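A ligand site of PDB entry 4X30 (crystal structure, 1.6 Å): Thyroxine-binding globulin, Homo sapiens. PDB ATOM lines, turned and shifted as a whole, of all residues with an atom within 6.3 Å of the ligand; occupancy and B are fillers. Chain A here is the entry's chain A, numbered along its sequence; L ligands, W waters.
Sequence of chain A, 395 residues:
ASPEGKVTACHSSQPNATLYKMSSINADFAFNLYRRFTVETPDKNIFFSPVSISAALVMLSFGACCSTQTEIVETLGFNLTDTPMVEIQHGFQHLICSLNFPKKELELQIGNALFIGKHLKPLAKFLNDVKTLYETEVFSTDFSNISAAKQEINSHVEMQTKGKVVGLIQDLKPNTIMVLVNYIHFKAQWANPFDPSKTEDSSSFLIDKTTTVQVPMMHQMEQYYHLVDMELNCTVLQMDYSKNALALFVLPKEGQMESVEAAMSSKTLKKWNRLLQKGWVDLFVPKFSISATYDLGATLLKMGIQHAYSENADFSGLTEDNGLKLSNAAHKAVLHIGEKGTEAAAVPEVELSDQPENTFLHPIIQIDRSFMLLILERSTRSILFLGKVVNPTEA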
ATOM      1  N   SER A  23      -7.598 -16.026   9.431  1.00  0.00           N
ATOM      2  CA  SER A  23      -7.553 -14.552   9.417  1.00  0.00           C
ATOM      3  C   SER A  23      -6.878 -13.996   8.165  1.00  0.00           C
ATOM      4  O   SER A  23      -7.425 -13.105   7.503  1.00  0.00           O
ATOM      5  CB  SER A  23      -6.919 -13.993  10.714  1.00  0.00           C
ATOM      6  OG  SER A  23      -5.585 -14.403  10.867  1.00  0.00           O
ATOM      7  N   SER A  24      -5.694 -14.512   7.837  1.00  0.00           N
ATOM      8  CA  SER A  24      -4.945 -14.056   6.663  1.00  0.00           C
ATOM      9  C   SER A  24      -5.679 -14.409   5.368  1.00  0.00           C
ATOM     10  O   SER A  24      -5.788 -13.574   4.459  1.00  0.00           O
ATOM     11  CB  SER A  24      -3.526 -14.651   6.667  1.00  0.00           C
ATOM     12  OG  SER A  24      -2.756 -14.099   7.731  1.00  0.00           O
ATOM     13  N   ILE A  25      -6.253 -15.613   5.307  1.00  0.00           N
ATOM     14  CA  ILE A  25      -6.995 -16.043   4.120  1.00  0.00           C
ATOM     15  C   ILE A  25      -8.250 -15.178   3.924  1.00  0.00           C
ATOM     16  O   ILE A  25      -8.533 -14.708   2.826  1.00  0.00           O
ATOM     17  CB  ILE A  25      -7.342 -17.535   4.216  1.00  0.00           C
ATOM     18  CG1 ILE A  25      -6.041 -18.363   4.077  1.00  0.00           C
ATOM     19  CG2 ILE A  25      -8.345 -17.964   3.132  1.00  0.00           C
ATOM     20  CD1 ILE A  25      -6.207 -19.759   4.572  1.00  0.00           C
ATOM     21  N   ALA A  27      -8.733 -12.168   4.993  1.00  0.00           N
ATOM     22  CA  ALA A  27      -8.311 -10.806   4.660  1.00  0.00           C
ATOM     23  C   ALA A  27      -7.933 -10.708   3.192  1.00  0.00           C
ATOM     24  O   ALA A  27      -8.325  -9.774   2.499  1.00  0.00           O
ATOM     25  CB  ALA A  27      -7.140 -10.356   5.536  1.00  0.00           C
ATOM     26  N   GLN A 238      -5.179   4.678  13.087  1.00  0.00           N
ATOM     27  CA  GLN A 238      -5.959   3.698  13.834  1.00  0.00           C
ATOM     28  C   GLN A 238      -6.806   4.430  14.884  1.00  0.00           C
ATOM     29  O   GLN A 238      -6.259   5.227  15.648  1.00  0.00           O
ATOM     30  CB  GLN A 238      -5.020   2.729  14.522  1.00  0.00           C
ATOM     31  CG  GLN A 238      -5.689   1.700  15.433  1.00  0.00           C
ATOM     32  CD  GLN A 238      -4.686   0.866  16.181  1.00  0.00           C
ATOM     33  OE1 GLN A 238      -3.574   0.643  15.690  1.00  0.00           O
ATOM     34  NE2 GLN A 238      -5.037   0.434  17.384  1.00  0.00           N
ATOM     35  N   ASP A 240      -9.507   3.297  17.843  1.00  0.00           N
ATOM     36  CA  ASP A 240     -10.078   2.156  18.522  1.00  0.00           C
ATOM     37  C   ASP A 240     -11.502   2.418  18.948  1.00  0.00           C
ATOM     38  O   ASP A 240     -11.840   3.508  19.373  1.00  0.00           O
ATOM     39  CB  ASP A 240      -9.285   1.824  19.779  1.00  0.00           C
ATOM     40  CG  ASP A 240      -7.922   1.234  19.475  1.00  0.00           C
ATOM     41  OD1 ASP A 240      -7.595   0.976  18.307  1.00  0.00           O
ATOM     42  OD2 ASP A 240      -7.181   1.016  20.454  1.00  0.00           O
ATOM     43  N   LEU A 246     -11.693  -1.930  15.941  1.00  0.00           N
ATOM     44  CA  LEU A 246     -10.958  -0.706  15.625  1.00  0.00           C
ATOM     45  C   LEU A 246     -11.152  -0.330  14.171  1.00  0.00           C
ATOM     46  O   LEU A 246     -11.512  -1.164  13.349  1.00  0.00           O
ATOM     47  CB  LEU A 246      -9.457  -0.853  15.904  1.00  0.00           C
ATOM     48  CG  LEU A 246      -8.787  -1.988  15.130  1.00  0.00           C
ATOM     49  CD1 LEU A 246      -7.425  -1.590  14.594  1.00  0.00           C
ATOM     50  CD2 LEU A 246      -8.756  -3.266  15.946  1.00  0.00           C
ATOM     51  N   LEU A 248      -9.358   1.477  10.810  1.00  0.00           N
ATOM     52  CA  LEU A 248      -8.204   2.016  10.105  1.00  0.00           C
ATOM     53  C   LEU A 248      -8.670   2.915   8.981  1.00  0.00           C
ATOM     54  O   LEU A 248      -9.429   2.481   8.108  1.00  0.00           O
ATOM     55  CB  LEU A 248      -7.370   0.910   9.496  1.00  0.00           C
ATOM     56  CG  LEU A 248      -6.671  -0.067  10.416  1.00  0.00           C
ATOM     57  CD1 LEU A 248      -5.863  -1.047   9.566  1.00  0.00           C
ATOM     58  CD2 LEU A 248      -5.793   0.647  11.413  1.00  0.00           C
ATOM     59  N   SER A 266      -3.202  -9.195   3.099  1.00  0.00           N
ATOM     60  CA  SER A 266      -2.908  -9.604   4.461  1.00  0.00           C
ATOM     61  C   SER A 266      -1.453  -9.266   4.817  1.00  0.00           C
ATOM     62  O   SER A 266      -1.178  -8.925   5.956  1.00  0.00           O
ATOM     63  CB  SER A 266      -3.191 -11.103   4.676  1.00  0.00           C
ATOM     64  OG  SER A 266      -2.297 -11.935   3.959  1.00  0.00           O
ATOM     65  N   THR A 268       0.176  -6.599   3.772  1.00  0.00           N
ATOM     66  CA  THR A 268       0.179  -5.179   4.119  1.00  0.00           C
ATOM     67  C   THR A 268      -0.310  -4.934   5.538  1.00  0.00           C
ATOM     68  O   THR A 268       0.222  -4.105   6.233  1.00  0.00           O
ATOM     69  CB  THR A 268      -0.693  -4.383   3.131  1.00  0.00           C
ATOM     70  OG1 THR A 268      -0.185  -4.609   1.812  1.00  0.00           O
ATOM     71  CG2 THR A 268      -0.662  -2.908   3.424  1.00  0.00           C
ATOM     72  N   LEU A 269      -1.348  -5.651   5.963  1.00  0.00           N
ATOM     73  CA  LEU A 269      -1.837  -5.514   7.328  1.00  0.00           C
ATOM     74  C   LEU A 269      -0.795  -5.950   8.323  1.00  0.00           C
ATOM     75  O   LEU A 269      -0.598  -5.276   9.308  1.00  0.00           O
ATOM     76  CB  LEU A 269      -3.136  -6.277   7.531  1.00  0.00           C
ATOM     77  CG  LEU A 269      -4.357  -5.799   6.756  1.00  0.00           C
ATOM     78  CD1 LEU A 269      -5.578  -6.637   7.112  1.00  0.00           C
ATOM     79  CD2 LEU A 269      -4.622  -4.310   6.984  1.00  0.00           C
ATOM     80  N   LYS A 270      -0.093  -7.046   8.056  1.00  0.00           N
ATOM     81  CA  LYS A 270       0.991  -7.450   8.936  1.00  0.00           C
ATOM     82  C   LYS A 270       2.077  -6.385   9.051  1.00  0.00           C
ATOM     83  O   LYS A 270       2.611  -6.121  10.149  1.00  0.00           O
ATOM     84  CB  LYS A 270       1.555  -8.792   8.512  1.00  0.00           C
ATOM     85  CG  LYS A 270       0.626  -9.927   8.917  1.00  0.00           C
ATOM     86  CD  LYS A 270       0.750 -11.133   8.014  1.00  0.00           C
ATOM     87  CE  LYS A 270      -0.457 -12.055   8.180  1.00  0.00           C
ATOM     88  NZ  LYS A 270      -1.760 -11.347   7.939  1.00  0.00           N
ATOM     89  N   TRP A 272       1.766  -3.104   8.564  1.00  0.00           N
ATOM     90  CA  TRP A 272       1.254  -1.998   9.348  1.00  0.00           C
ATOM     91  C   TRP A 272       1.162  -2.339  10.835  1.00  0.00           C
ATOM     92  O   TRP A 272       1.422  -1.483  11.671  1.00  0.00           O
ATOM     93  CB  TRP A 272      -0.100  -1.546   8.823  1.00  0.00           C
ATOM     94  CG  TRP A 272      -0.044  -0.942   7.448  1.00  0.00           C
ATOM     95  CD1 TRP A 272       1.065  -0.546   6.753  1.00  0.00           C
ATOM     96  CD2 TRP A 272      -1.169  -0.601   6.638  1.00  0.00           C
ATOM     97  NE1 TRP A 272       0.696   0.000   5.561  1.00  0.00           N
ATOM     98  CE2 TRP A 272      -0.666  -0.031   5.459  1.00  0.00           C
ATOM     99  CE3 TRP A 272      -2.553  -0.721   6.799  1.00  0.00           C
ATOM    100  CZ2 TRP A 272      -1.514   0.425   4.429  1.00  0.00           C
ATOM    101  CZ3 TRP A 272      -3.381  -0.260   5.777  1.00  0.00           C
ATOM    102  CH2 TRP A 272      -2.853   0.304   4.624  1.00  0.00           C
ATOM    103  N   ASN A 273       0.803  -3.565  11.170  1.00  0.00           N
ATOM    104  CA  ASN A 273       0.703  -3.970  12.570  1.00  0.00           C
ATOM    105  C   ASN A 273       2.013  -3.745  13.299  1.00  0.00           C
ATOM    106  O   ASN A 273       2.007  -3.296  14.445  1.00  0.00           O
ATOM    107  CB  ASN A 273       0.267  -5.433  12.686  1.00  0.00           C
ATOM    108  CG  ASN A 273      -0.135  -5.799  14.095  1.00  0.00           C
ATOM    109  OD1 ASN A 273      -1.272  -5.563  14.492  1.00  0.00           O
ATOM    110  ND2 ASN A 273       0.761  -6.433  14.816  1.00  0.00           N
ATOM    111  N   LEU A 276       2.930   0.663  12.867  1.00  0.00           N
ATOM    112  CA  LEU A 276       2.114   1.684  13.538  1.00  0.00           C
ATOM    113  C   LEU A 276       2.772   2.134  14.836  1.00  0.00           C
ATOM    114  O   LEU A 276       3.195   1.300  15.632  1.00  0.00           O
ATOM    115  CB  LEU A 276       0.716   1.125  13.803  1.00  0.00           C
ATOM    116  CG  LEU A 276      -0.207   1.070  12.580  1.00  0.00           C
ATOM    117  CD1 LEU A 276      -1.333   0.120  12.857  1.00  0.00           C
ATOM    118  CD2 LEU A 276      -0.786   2.443  12.246  1.00  0.00           C
ATOM    119  N   LEU A 376     -11.870  -3.561  11.856  1.00  0.00           N
ATOM    120  CA  LEU A 376     -11.277  -4.837  12.203  1.00  0.00           C
ATOM    121  C   LEU A 376     -11.701  -5.281  13.608  1.00  0.00           C
ATOM    122  O   LEU A 376     -11.953  -4.449  14.482  1.00  0.00           O
ATOM    123  CB  LEU A 376      -9.744  -4.743  12.182  1.00  0.00           C
ATOM    124  CG  LEU A 376      -9.113  -4.161  10.911  1.00  0.00           C
ATOM    125  CD1 LEU A 376      -7.621  -3.899  11.004  1.00  0.00           C
ATOM    126  CD2 LEU A 376      -9.395  -5.074   9.751  1.00  0.00           C
ATOM    127  N   GLU A 377     -11.747  -6.583  13.819  1.00  0.00           N
ATOM    128  CA  GLU A 377     -12.112  -7.147  15.107  1.00  0.00           C
ATOM    129  C   GLU A 377     -10.866  -7.861  15.593  1.00  0.00           C
ATOM    130  O   GLU A 377     -10.306  -8.663  14.883  1.00  0.00           O
ATOM    131  CB  GLU A 377     -13.318  -8.079  14.982  1.00  0.00           C
ATOM    132  CG  GLU A 377     -13.960  -8.501  16.298  1.00  0.00           C
ATOM    133  CD  GLU A 377     -13.129  -9.526  17.032  1.00  0.00           C
ATOM    134  OE1 GLU A 377     -12.563 -10.399  16.341  1.00  0.00           O
ATOM    135  OE2 GLU A 377     -13.016  -9.445  18.286  1.00  0.00           O
ATOM    136  N   ARG A 378     -10.452  -7.536  16.816  1.00  0.00           N
ATOM    137  CA  ARG A 378      -9.188  -7.941  17.372  1.00  0.00           C
ATOM    138  C   ARG A 378      -9.021  -9.404  17.765  1.00  0.00           C
ATOM    139  O   ARG A 378      -7.954  -9.985  17.537  1.00  0.00           O
ATOM    140  CB  ARG A 378      -8.950  -7.084  18.630  1.00  0.00           C
ATOM    141  CG  ARG A 378      -7.526  -6.805  18.991  1.00  0.00           C
ATOM    142  CD  ARG A 378      -7.460  -5.863  20.187  1.00  0.00           C
ATOM    143  NE  ARG A 378      -8.017  -4.524  19.945  1.00  0.00           N
ATOM    144  CZ  ARG A 378      -7.294  -3.405  19.801  1.00  0.00           C
ATOM    145  NH1 ARG A 378      -5.963  -3.436  19.835  1.00  0.00           N
ATOM    146  NH2 ARG A 378      -7.903  -2.252  19.638  1.00  0.00           N
ATOM    147  N   SER A 379     -10.048  -9.996  18.387  1.00  0.00           N
ATOM    148  CA  SER A 379      -9.908 -11.339  18.952  1.00  0.00           C
ATOM    149  C   SER A 379      -9.765 -12.396  17.881  1.00  0.00           C
ATOM    150  O   SER A 379      -9.136 -13.427  18.111  1.00  0.00           O
ATOM    151  CB  SER A 379     -11.084 -11.691  19.871  1.00  0.00           C
ATOM    152  OG  SER A 379     -12.310 -11.797  19.186  1.00  0.00           O
ATOM    153  N   THR A 380     -10.327 -12.133  16.711  1.00  0.00           N
ATOM    154  CA  THR A 380     -10.312 -13.111  15.620  1.00  0.00           C
ATOM    155  C   THR A 380      -9.564 -12.594  14.386  1.00  0.00           C
ATOM    156  O   THR A 380      -9.400 -13.356  13.425  1.00  0.00           O
ATOM    157  CB  THR A 380     -11.741 -13.460  15.146  1.00  0.00           C
ATOM    158  OG1 THR A 380     -12.346 -12.308  14.543  1.00  0.00           O
ATOM    159  CG2 THR A 380     -12.607 -13.957  16.303  1.00  0.00           C
ATOM    160  N   ARG A 381      -9.148 -11.335  14.394  1.00  0.00           N
ATOM    161  CA  ARG A 381      -8.501 -10.667  13.250  1.00  0.00           C
ATOM    162  C   ARG A 381      -9.382 -10.736  12.006  1.00  0.00           C
ATOM    163  O   ARG A 381      -8.888 -10.974  10.902  1.00  0.00           O
ATOM    164  CB  ARG A 381      -7.104 -11.214  12.968  1.00  0.00           C
ATOM    165  CG  ARG A 381      -6.108 -10.885  14.062  1.00  0.00           C
ATOM    166  CD  ARG A 381      -4.772 -11.525  13.746  1.00  0.00           C
ATOM    167  NE  ARG A 381      -3.801 -11.202  14.795  1.00  0.00           N
ATOM    168  CZ  ARG A 381      -2.622 -11.781  14.916  1.00  0.00           C
ATOM    169  NH1 ARG A 381      -1.815 -11.400  15.888  1.00  0.00           N
ATOM    170  NH2 ARG A 381      -2.226 -12.718  14.061  1.00  0.00           N
ATOM    171  N   SER A 382     -10.668 -10.486  12.185  1.00  0.00           N
ATOM    172  CA  SER A 382     -11.623 -10.459  11.063  1.00  0.00           C
ATOM    173  C   SER A 382     -11.814  -9.034  10.581  1.00  0.00           C
ATOM    174  O   SER A 382     -11.757  -8.085  11.363  1.00  0.00           O
ATOM    175  CB  SER A 382     -12.974 -11.000  11.504  1.00  0.00           C
ATOM    176  OG  SER A 382     -12.903 -12.378  11.807  1.00  0.00           O
ATOM    177  N   ILE A 383     -12.102  -8.896   9.296  1.00  0.00           N
ATOM    178  CA  ILE A 383     -12.455  -7.607   8.729  1.00  0.00           C
ATOM    179  C   ILE A 383     -13.980  -7.546   8.726  1.00  0.00           C
ATOM    180  O   ILE A 383     -14.660  -8.215   7.958  1.00  0.00           O
ATOM    181  CB  ILE A 383     -11.906  -7.412   7.314  1.00  0.00           C
ATOM    182  CG1 ILE A 383     -10.385  -7.640   7.301  1.00  0.00           C
ATOM    183  CG2 ILE A 383     -12.262  -6.020   6.808  1.00  0.00           C
ATOM    184  CD1 ILE A 383      -9.721  -7.428   5.960  1.00  0.00           C
HETATM  185  C1  LIG L   1      -4.353  -3.861  15.229  1.00  0.00           C
HETATM  186  C2  LIG L   1      -5.284  -4.877  15.228  1.00  0.00           C
HETATM  187  C3  LIG L   1      -5.603  -5.577  14.067  1.00  0.00           C
HETATM  188  C4  LIG L   1      -4.923  -5.244  12.814  1.00  0.00           C
HETATM  189  C5  LIG L   1      -3.941  -4.161  12.891  1.00  0.00           C
HETATM  190  C6  LIG L   1      -3.678  -3.477  14.065  1.00  0.00           C
HETATM  191  C7  LIG L   1      -4.049  -3.174  16.545  1.00  0.00           C
HETATM  192  C8  LIG L   1      -3.197  -4.084  17.473  1.00  0.00           C
HETATM  193  C9  LIG L   1      -3.834  -5.442  17.804  1.00  0.00           C
HETATM  194  C10 LIG L   1      -4.451  -7.100  11.418  1.00  0.00           C
HETATM  195  C11 LIG L   1      -3.212  -7.429  12.025  1.00  0.00           C
HETATM  196  C12 LIG L   1      -2.563  -8.632  11.728  1.00  0.00           C
HETATM  197  C13 LIG L   1      -3.152  -9.594  10.796  1.00  0.00           C
HETATM  198  C14 LIG L   1      -4.426  -9.199  10.220  1.00  0.00           C
HETATM  199  C15 LIG L   1      -5.027  -7.992  10.543  1.00  0.00           C
HETATM  200  N1  LIG L   1      -1.893  -4.286  16.886  1.00  0.00           N
HETATM  201  O1  LIG L   1      -5.155  -5.915  11.655  1.00  0.00           O
HETATM  202  O2  LIG L   1      -2.529 -10.770  10.497  1.00  0.00           O
HETATM  203  O3  LIG L   1      -3.526  -6.538  17.238  1.00  0.00           O
HETATM  204  O4  LIG L   1      -4.700  -5.436  18.678  1.00  0.00           O
HETATM  205  I1  LIG L   1      -7.085  -7.030  14.134  1.00  0.00           I
HETATM  206  I2  LIG L   1      -0.727  -9.199  12.541  1.00  0.00           I
HETATM  207  I3  LIG L   1      -3.030  -3.641  11.116  1.00  0.00           I
HETATM  208  I4  LIG L   1      -5.271 -10.570   8.911  1.00  0.00           I
HETATM  209  O   HOH W   1      -0.573  -2.652  15.625  1.00  0.00           O
HETATM  210  O   HOH W   2      -4.994  -9.151  16.915  1.00  0.00           O
HETATM  211  O   HOH W   3      -1.160  -7.978  16.768  1.00  0.00           O
HETATM  212  O   HOH W   4      -8.072  -8.660  10.197  1.00  0.00           O
HETATM  213  O   HOH W   5      -3.224 -13.149  11.217  1.00  0.00           O
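NH2 of Arg 378 lies within salt-bridge range of OD2 of Asp 240, 3.4 Å away.
NZ of Lys 270 is in hydrogen-bond range of OG of Ser 24, 2.9 Å away.
O of Ser 266 lies within hydrogen-bond range of NZ of Lys 270 (3.2 Å).
The backbone carbonyl oxygen (O) of Leu 246 sits at hydrogen-bond distance from the backbone NH (N) of Leu 376.
N of Glu 377 is in hydrogen-bond range of O of Ser 382 (2.9 Å).
The side-chain hydroxyl (OG) of Ser 379 lies within hydrogen-bond range of the side-chain carboxylate (OE2) of Glu 377, 2.6 Å away.
OE1 of Glu 377 lies within hydrogen-bond range of OG1 of Thr 380 (2.6 Å).
The side-chain amide nitrogen (NE2) of Gln 238 lies within hydrogen-bond range of the side-chain carboxylate (OD1) of Asp 240 (2.8 Å).
Water W1 lies within hydrogen-bond range of a nitrogen (N1) of the ligand (2.4 Å) and the backbone carbonyl oxygen (O) of Asn 273 (2.9 Å).
Water W5 lies within hydrogen-bond range of O2 of the ligand (2.6 Å), OG of Ser 23 (2.7 Å) and NH2 of Arg 381 (3.0 Å).
Water W3 lies within hydrogen-bond range of O3 of the ligand (2.8 Å) and ND2 of Asn 273 (3.1 Å).
Water W2 lies within hydrogen-bond range of an oxygen (O3) of the ligand (3.0 Å), the backbone carbonyl oxygen of Arg 378 (3.1 Å) and the guanidinium group of Arg 381 (3.2 Å).
NH1 of Arg 378 lies within salt-bridge range of O4 of the ligand.
An oxygen (O2) of the ligand sits at hydrogen-bond distance from the side-chain amino group (NZ) of Lys 270.
The side-chain amide oxygen (OD1) of Asn 273 sits at hydrogen-bond distance from a nitrogen (N1) of the ligand (2.8 Å).
O of Ser 23 touches I4 of the ligand (3.6 Å).
Ala 27 touches the ligand.
Gln 238 touches the ligand.
Leu 246 touches the ligand.
O of Leu 269 touches I3 of the ligand, 3.4 Å away.
CD1 of Leu 376 touches O1 of the ligand, 3.3 Å away.
Glu 377 touches the ligand (O to I1, 3.7 Å).
Arg 381 touches the ligand (CD to C13, 3.9 Å).
Hydrophobic or aromatic side chains within 4 Å of the ligand: Ala 27, Leu 246, Leu 269 and Leu 376.
Within 4 Å of the ligand: Ser 23, Ala 27, Gln 238, Leu 246, Leu 269, Lys 270, Asn 273, Leu 376, Glu 377, Arg 378 and Arg 381.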
